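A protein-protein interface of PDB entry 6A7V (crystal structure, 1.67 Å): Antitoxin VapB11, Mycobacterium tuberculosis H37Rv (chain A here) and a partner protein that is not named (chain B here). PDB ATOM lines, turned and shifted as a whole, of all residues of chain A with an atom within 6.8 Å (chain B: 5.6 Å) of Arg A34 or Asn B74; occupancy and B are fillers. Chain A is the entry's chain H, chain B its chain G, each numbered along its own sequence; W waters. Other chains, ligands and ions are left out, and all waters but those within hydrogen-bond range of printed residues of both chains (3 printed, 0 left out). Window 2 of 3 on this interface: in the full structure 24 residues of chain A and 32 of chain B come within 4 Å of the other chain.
NH2 of Arg B112 lies within hydrogen-bond range of O of Asn B74, 2.8 Å away. OD1 of Asn B74 is in hydrogen-bond range of NE2 of His B113 (3.0 Å).
N of Ser B72 sits at hydrogen-bond distance from O of Arg A34, 3.1 Å away.
Printed residues of chain A that touch a printed residue of chain B: Arg A34, Leu A35, Val A36 and Gly A37. Printed residues of chain B that touch a printed residue of chain A: Leu B70, Pro B71, Ser B72 and Asn B74. Hydrophobic or aromatic side chains of chain B within 4 Å of the printed part of chain A: Pro B71. Among the printed residues, no Asp or Glu carboxylate lies within 4 Å of a Lys or Arg side-chain nitrogen of the other chain.
Ala A31 touches none of the printed residues of chain B. Of the printed residues of chain B, Val A36 touches Pro B71. Printed residues of chain A within 4 Å of Pro B71: Arg A34, Leu A35, Val A36 and Gly A37. Of chain A, only Arg A34 (3.8 Å) comes within 4 Å of Asn B74. The nearest residue of chain B that does not touch Arg A34 is Leu B70 (5.3 Å).
O of Arg A34 touches CA of Pro B71 (3.4 Å). NH2 of Arg A34 touches CB of Asn B74, 3.8 Å away. Leu A35 touches Pro B71. Pro B71 touches Val A36 (CG to C, 3.7 Å). Gly A37 touches Leu B70. Gly A37 touches Pro B71.
Water W3 lies within hydrogen-bond range of the backbone carbonyl oxygen (O) of Arg A33 (2.6 Å), the backbone carbonyl oxygen (O) of Leu B70 (2.7 Å) and the backbone NH (N) of Ser B72 (3.4 Å). Water W1 lies within hydrogen-bond range of the backbone carbonyl oxygen of Arg A34 and the backbone carbonyl oxygen of Ser B72. Water W2 lies within hydrogen-bond range of the guanidinium group (NH2) of Arg A34 (3.0 Å) and the side-chain amide nitrogen (ND2) of Asn B74 (3.2 Å).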
ATOM      1  N   PHE A  19      10.354  -3.349   9.238  1.00  0.00           N
ATOM      2  CA  PHE A  19       9.893  -3.092  10.608  1.00  0.00           C
ATOM      3  C   PHE A  19       9.376  -1.665  10.815  1.00  0.00           C
ATOM      4  O   PHE A  19       9.123  -1.258  11.954  1.00  0.00           O
ATOM      5  CB  PHE A  19      11.024  -3.395  11.596  1.00  0.00           C
ATOM      6  CG  PHE A  19      11.338  -4.859  11.709  1.00  0.00           C
ATOM      7  CD1 PHE A  19      12.143  -5.483  10.765  1.00  0.00           C
ATOM      8  CD2 PHE A  19      10.812  -5.620  12.747  1.00  0.00           C
ATOM      9  CE1 PHE A  19      12.425  -6.835  10.857  1.00  0.00           C
ATOM     10  CE2 PHE A  19      11.093  -6.971  12.846  1.00  0.00           C
ATOM     11  CZ  PHE A  19      11.899  -7.580  11.900  1.00  0.00           C
ATOM     12  N   ASP A  29      19.697  -1.709  17.078  1.00  0.00           N
ATOM     13  CA  ASP A  29      19.243  -1.898  18.438  1.00  0.00           C
ATOM     14  C   ASP A  29      18.329  -3.106  18.436  1.00  0.00           C
ATOM     15  O   ASP A  29      18.550  -4.018  19.191  1.00  0.00           O
ATOM     16  CB  ASP A  29      18.467  -0.688  18.986  1.00  0.00           C
ATOM     17  CG  ASP A  29      19.359   0.326  19.701  1.00  0.00           C
ATOM     18  OD1 ASP A  29      20.597   0.155  19.721  1.00  0.00           O
ATOM     19  OD2 ASP A  29      18.808   1.308  20.248  1.00  0.00           O
ATOM     20  N   LEU A  30      17.316  -3.087  17.572  1.00  0.00           N
ATOM     21  CA  LEU A  30      16.339  -4.162  17.517  1.00  0.00           C
ATOM     22  C   LEU A  30      17.087  -5.473  17.260  1.00  0.00           C
ATOM     23  O   LEU A  30      16.967  -6.372  18.032  1.00  0.00           O
ATOM     24  CB  LEU A  30      15.319  -3.912  16.402  1.00  0.00           C
ATOM     25  CG  LEU A  30      14.324  -5.038  16.101  1.00  0.00           C
ATOM     26  CD1 LEU A  30      13.471  -5.345  17.321  1.00  0.00           C
ATOM     27  CD2 LEU A  30      13.453  -4.681  14.906  1.00  0.00           C
ATOM     28  N   ALA A  31      17.904  -5.470  16.195  1.00  0.00           N
ATOM     29  CA  ALA A  31      18.635  -6.622  15.765  1.00  0.00           C
ATOM     30  C   ALA A  31      19.329  -7.289  16.965  1.00  0.00           C
ATOM     31  O   ALA A  31      19.408  -8.499  17.033  1.00  0.00           O
ATOM     32  CB  ALA A  31      19.654  -6.251  14.697  1.00  0.00           C
ATOM     33  N   LEU A  32      19.934  -6.469  17.823  1.00  0.00           N
ATOM     34  CA  LEU A  32      20.699  -6.976  18.921  1.00  0.00           C
ATOM     35  C   LEU A  32      19.773  -7.444  20.060  1.00  0.00           C
ATOM     36  O   LEU A  32      20.045  -8.457  20.691  1.00  0.00           O
ATOM     37  CB  LEU A  32      21.744  -5.963  19.410  1.00  0.00           C
ATOM     38  CG  LEU A  32      22.909  -5.705  18.443  1.00  0.00           C
ATOM     39  CD1 LEU A  32      23.852  -4.664  19.028  1.00  0.00           C
ATOM     40  CD2 LEU A  32      23.670  -6.980  18.102  1.00  0.00           C
ATOM     41  N   ARG A  33      18.758  -6.672  20.353  1.00  0.00           N
ATOM     42  CA  ARG A  33      17.852  -7.000  21.426  1.00  0.00           C
ATOM     43  C   ARG A  33      17.166  -8.338  21.177  1.00  0.00           C
ATOM     44  O   ARG A  33      17.020  -9.132  22.097  1.00  0.00           O
ATOM     45  CB  ARG A  33      16.796  -5.889  21.578  1.00  0.00           C
ATOM     46  CG  ARG A  33      15.805  -6.090  22.723  1.00  0.00           C
ATOM     47  CD  ARG A  33      14.498  -5.336  22.504  1.00  0.00           C
ATOM     48  NE  ARG A  33      13.361  -6.005  23.145  1.00  0.00           N
ATOM     49  CZ  ARG A  33      12.685  -7.037  22.630  1.00  0.00           C
ATOM     50  NH1 ARG A  33      11.671  -7.566  23.310  1.00  0.00           N
ATOM     51  NH2 ARG A  33      13.012  -7.556  21.447  1.00  0.00           N
ATOM     52  N   ARG A  34      16.748  -8.557  19.918  1.00  0.00           N
ATOM     53  CA  ARG A  34      16.071  -9.766  19.545  1.00  0.00           C
ATOM     54  C   ARG A  34      17.025 -10.961  19.819  1.00  0.00           C
ATOM     55  O   ARG A  34      16.581 -12.007  20.340  1.00  0.00           O
ATOM     56  CB  ARG A  34      15.624  -9.787  18.084  1.00  0.00           C
ATOM     57  CG  ARG A  34      15.013 -11.130  17.701  1.00  0.00           C
ATOM     58  CD  ARG A  34      14.455 -11.164  16.295  1.00  0.00           C
ATOM     59  NE  ARG A  34      13.183 -10.457  16.186  1.00  0.00           N
ATOM     60  CZ  ARG A  34      12.377 -10.513  15.127  1.00  0.00           C
ATOM     61  NH1 ARG A  34      12.695 -11.250  14.064  1.00  0.00           N
ATOM     62  NH2 ARG A  34      11.239  -9.826  15.130  1.00  0.00           N
ATOM     63  N   LEU A  35      18.315 -10.827  19.464  1.00  0.00           N
ATOM     64  CA  LEU A  35      19.152 -11.968  19.381  1.00  0.00           C
ATOM     65  C   LEU A  35      19.760 -12.368  20.715  1.00  0.00           C
ATOM     66  O   LEU A  35      19.905 -13.545  20.983  1.00  0.00           O
ATOM     67  CB  LEU A  35      20.268 -11.707  18.362  1.00  0.00           C
ATOM     68  CG  LEU A  35      21.155 -12.886  17.965  1.00  0.00           C
ATOM     69  CD1 LEU A  35      20.324 -14.046  17.436  1.00  0.00           C
ATOM     70  CD2 LEU A  35      22.172 -12.429  16.931  1.00  0.00           C
ATOM     71  N   VAL A  36      20.127 -11.386  21.533  1.00  0.00           N
ATOM     72  CA  VAL A  36      20.726 -11.654  22.846  1.00  0.00           C
ATOM     73  C   VAL A  36      20.049 -10.898  23.997  1.00  0.00           C
ATOM     74  O   VAL A  36      20.495 -10.994  25.140  1.00  0.00           O
ATOM     75  CB  VAL A  36      22.232 -11.313  22.853  1.00  0.00           C
ATOM     76  CG1 VAL A  36      23.010 -12.268  21.962  1.00  0.00           C
ATOM     77  CG2 VAL A  36      22.462  -9.873  22.422  1.00  0.00           C
ATOM     78  N   GLY A  37      18.982 -10.157  23.702  1.00  0.00           N
ATOM     79  CA  GLY A  37      18.277  -9.391  24.721  1.00  0.00           C
ATOM     80  C   GLY A  37      19.015  -8.143  25.157  1.00  0.00           C
ATOM     81  O   GLY A  37      19.850  -7.602  24.428  1.00  0.00           O
ATOM     82  N   SER A  38      18.681  -7.684  26.357  1.00  0.00           N
ATOM     83  CA  SER A  38      19.353  -6.568  26.998  1.00  0.00           C
ATOM     84  C   SER A  38      20.066  -7.127  28.217  1.00  0.00           C
ATOM     85  O   SER A  38      19.704  -8.206  28.695  1.00  0.00           O
ATOM     86  CB  SER A  38      18.339  -5.506  27.427  1.00  0.00           C
ATOM     87  OG  SER A  38      17.489  -5.136  26.354  1.00  0.00           O
ATOM     88  N   LEU B  70      15.026 -10.431  27.806  1.00  0.00           N
ATOM     89  CA  LEU B  70      15.354 -11.734  27.244  1.00  0.00           C
ATOM     90  C   LEU B  70      15.326 -11.709  25.718  1.00  0.00           C
ATOM     91  O   LEU B  70      14.558 -10.952  25.123  1.00  0.00           O
ATOM     92  CB  LEU B  70      14.386 -12.800  27.760  1.00  0.00           C
ATOM     93  CG  LEU B  70      14.489 -13.169  29.245  1.00  0.00           C
ATOM     94  CD1 LEU B  70      13.309 -14.028  29.658  1.00  0.00           C
ATOM     95  CD2 LEU B  70      15.795 -13.892  29.539  1.00  0.00           C
ATOM     96  N   PRO B  71      16.163 -12.548  25.076  1.00  0.00           N
ATOM     97  CA  PRO B  71      16.055 -12.737  23.632  1.00  0.00           C
ATOM     98  C   PRO B  71      14.656 -13.216  23.286  1.00  0.00           C
ATOM     99  O   PRO B  71      14.082 -14.009  24.036  1.00  0.00           O
ATOM    100  CB  PRO B  71      17.079 -13.838  23.322  1.00  0.00           C
ATOM    101  CG  PRO B  71      17.970 -13.918  24.505  1.00  0.00           C
ATOM    102  CD  PRO B  71      17.236 -13.355  25.680  1.00  0.00           C
ATOM    103  N   SER B  72      14.121 -12.743  22.164  1.00  0.00           N
ATOM    104  CA  SER B  72      12.747 -13.050  21.782  1.00  0.00           C
ATOM    105  C   SER B  72      12.665 -13.984  20.579  1.00  0.00           C
ATOM    106  O   SER B  72      13.396 -13.813  19.609  1.00  0.00           O
ATOM    107  CB  SER B  72      11.993 -11.768  21.456  1.00  0.00           C
ATOM    108  OG  SER B  72      10.637 -12.067  21.164  1.00  0.00           O
ATOM    109  N   LEU B  73      11.774 -14.971  20.666  1.00  0.00           N
ATOM    110  CA  LEU B  73      11.406 -15.812  19.533  1.00  0.00           C
ATOM    111  C   LEU B  73      10.108 -15.229  18.974  1.00  0.00           C
ATOM    112  O   LEU B  73       9.076 -15.260  19.648  1.00  0.00           O
ATOM    113  CB  LEU B  73      11.185 -17.255  19.991  1.00  0.00           C
ATOM    114  CG  LEU B  73      12.334 -17.917  20.759  1.00  0.00           C
ATOM    115  CD1 LEU B  73      11.985 -19.356  21.100  1.00  0.00           C
ATOM    116  CD2 LEU B  73      13.621 -17.859  19.951  1.00  0.00           C
ATOM    117  N   ASN B  74      10.169 -14.677  17.764  1.00  0.00           N
ATOM    118  CA  ASN B  74       9.043 -13.913  17.215  1.00  0.00           C
ATOM    119  C   ASN B  74       7.849 -14.794  16.822  1.00  0.00           C
ATOM    120  O   ASN B  74       7.996 -15.980  16.540  1.00  0.00           O
ATOM    121  CB  ASN B  74       9.480 -13.051  16.016  1.00  0.00           C
ATOM    122  CG  ASN B  74       9.732 -13.866  14.754  1.00  0.00           C
ATOM    123  OD1 ASN B  74      10.245 -14.970  14.812  1.00  0.00           O
ATOM    124  ND2 ASN B  74       9.373 -13.309  13.605  1.00  0.00           N
ATOM    125  N   VAL B  75       6.665 -14.197  16.852  1.00  0.00           N
ATOM    126  CA  VAL B  75       5.483 -14.759  16.214  1.00  0.00           C
ATOM    127  C   VAL B  75       5.447 -14.216  14.794  1.00  0.00           C
ATOM    128  O   VAL B  75       5.525 -13.004  14.587  1.00  0.00           O
ATOM    129  CB  VAL B  75       4.186 -14.346  16.949  1.00  0.00           C
ATOM    130  CG1 VAL B  75       2.952 -14.795  16.170  1.00  0.00           C
ATOM    131  CG2 VAL B  75       4.169 -14.929  18.350  1.00  0.00           C
ATOM    132  N   ASP B  76       5.334 -15.112  13.821  1.00  0.00           N
ATOM    133  CA  ASP B  76       5.220 -14.732  12.414  1.00  0.00           C
ATOM    134  C   ASP B  76       3.830 -15.147  11.948  1.00  0.00           C
ATOM    135  O   ASP B  76       3.570 -16.332  11.791  1.00  0.00           O
ATOM    136  CB  ASP B  76       6.301 -15.439  11.587  1.00  0.00           C
ATOM    137  CG  ASP B  76       6.306 -15.014  10.120  1.00  0.00           C
ATOM    138  OD1 ASP B  76       5.269 -14.514   9.622  1.00  0.00           O
ATOM    139  OD2 ASP B  76       7.359 -15.184   9.459  1.00  0.00           O
ATOM    140  N   ASP B  80       2.379 -19.082  12.052  1.00  0.00           N
ATOM    141  CA  ASP B  80       2.311 -19.684  13.373  1.00  0.00           C
ATOM    142  C   ASP B  80       0.864 -19.912  13.762  1.00  0.00           C
ATOM    143  O   ASP B  80       0.602 -20.914  14.430  1.00  0.00           O
ATOM    144  CB  ASP B  80       3.035 -18.837  14.424  1.00  0.00           C
ATOM    145  CG  ASP B  80       4.550 -18.802  14.219  1.00  0.00           C
ATOM    146  OD1 ASP B  80       5.121 -19.744  13.612  1.00  0.00           O
ATOM    147  OD2 ASP B  80       5.173 -17.822  14.676  1.00  0.00           O
ATOM    148  N   LEU B 109       5.416 -21.941  17.644  1.00  0.00           N
ATOM    149  CA  LEU B 109       6.546 -21.031  17.487  1.00  0.00           C
ATOM    150  C   LEU B 109       7.859 -21.715  17.936  1.00  0.00           C
ATOM    151  O   LEU B 109       8.859 -21.581  17.254  1.00  0.00           O
ATOM    152  CB  LEU B 109       6.313 -19.639  18.061  1.00  0.00           C
ATOM    153  CG  LEU B 109       6.318 -19.395  19.553  1.00  0.00           C
ATOM    154  CD1 LEU B 109       7.731 -19.168  20.076  1.00  0.00           C
ATOM    155  CD2 LEU B 109       5.434 -18.188  19.827  1.00  0.00           C
ATOM    156  N   ARG B 112       9.029 -24.025  15.254  1.00  0.00           N
ATOM    157  CA  ARG B 112       9.547 -23.244  14.158  1.00  0.00           C
ATOM    158  C   ARG B 112      10.997 -22.816  14.481  1.00  0.00           C
ATOM    159  O   ARG B 112      11.881 -22.885  13.603  1.00  0.00           O
ATOM    160  CB  ARG B 112       8.682 -22.057  13.761  1.00  0.00           C
ATOM    161  CG  ARG B 112       9.237 -21.330  12.538  1.00  0.00           C
ATOM    162  CD  ARG B 112       8.245 -20.359  11.932  1.00  0.00           C
ATOM    163  NE  ARG B 112       7.775 -19.374  12.903  1.00  0.00           N
ATOM    164  CZ  ARG B 112       8.426 -18.266  13.252  1.00  0.00           C
ATOM    165  NH1 ARG B 112       9.609 -17.952  12.721  1.00  0.00           N
ATOM    166  NH2 ARG B 112       7.886 -17.454  14.150  1.00  0.00           N
ATOM    167  N   HIS B 113      11.215 -22.368  15.724  1.00  0.00           N
ATOM    168  CA  HIS B 113      12.470 -21.768  16.072  1.00  0.00           C
ATOM    169  C   HIS B 113      13.556 -22.753  16.471  1.00  0.00           C
ATOM    170  O   HIS B 113      14.673 -22.374  16.728  1.00  0.00           O
ATOM    171  CB  HIS B 113      12.251 -20.740  17.181  1.00  0.00           C
ATOM    172  CG  HIS B 113      11.704 -19.433  16.700  1.00  0.00           C
ATOM    173  ND1 HIS B 113      12.489 -18.482  16.086  1.00  0.00           N
ATOM    174  CD2 HIS B 113      10.461 -18.896  16.779  1.00  0.00           C
ATOM    175  CE1 HIS B 113      11.752 -17.424  15.794  1.00  0.00           C
ATOM    176  NE2 HIS B 113      10.517 -17.648  16.207  1.00  0.00           N
HETATM  177  O   HOH W   1      16.120 -14.503  19.550  1.00  0.00           O
HETATM  178  O   HOH W   2       9.506 -10.253  12.773  1.00  0.00           O
HETATM  179  O   HOH W   3      14.528  -9.424  22.939  1.00  0.00           O
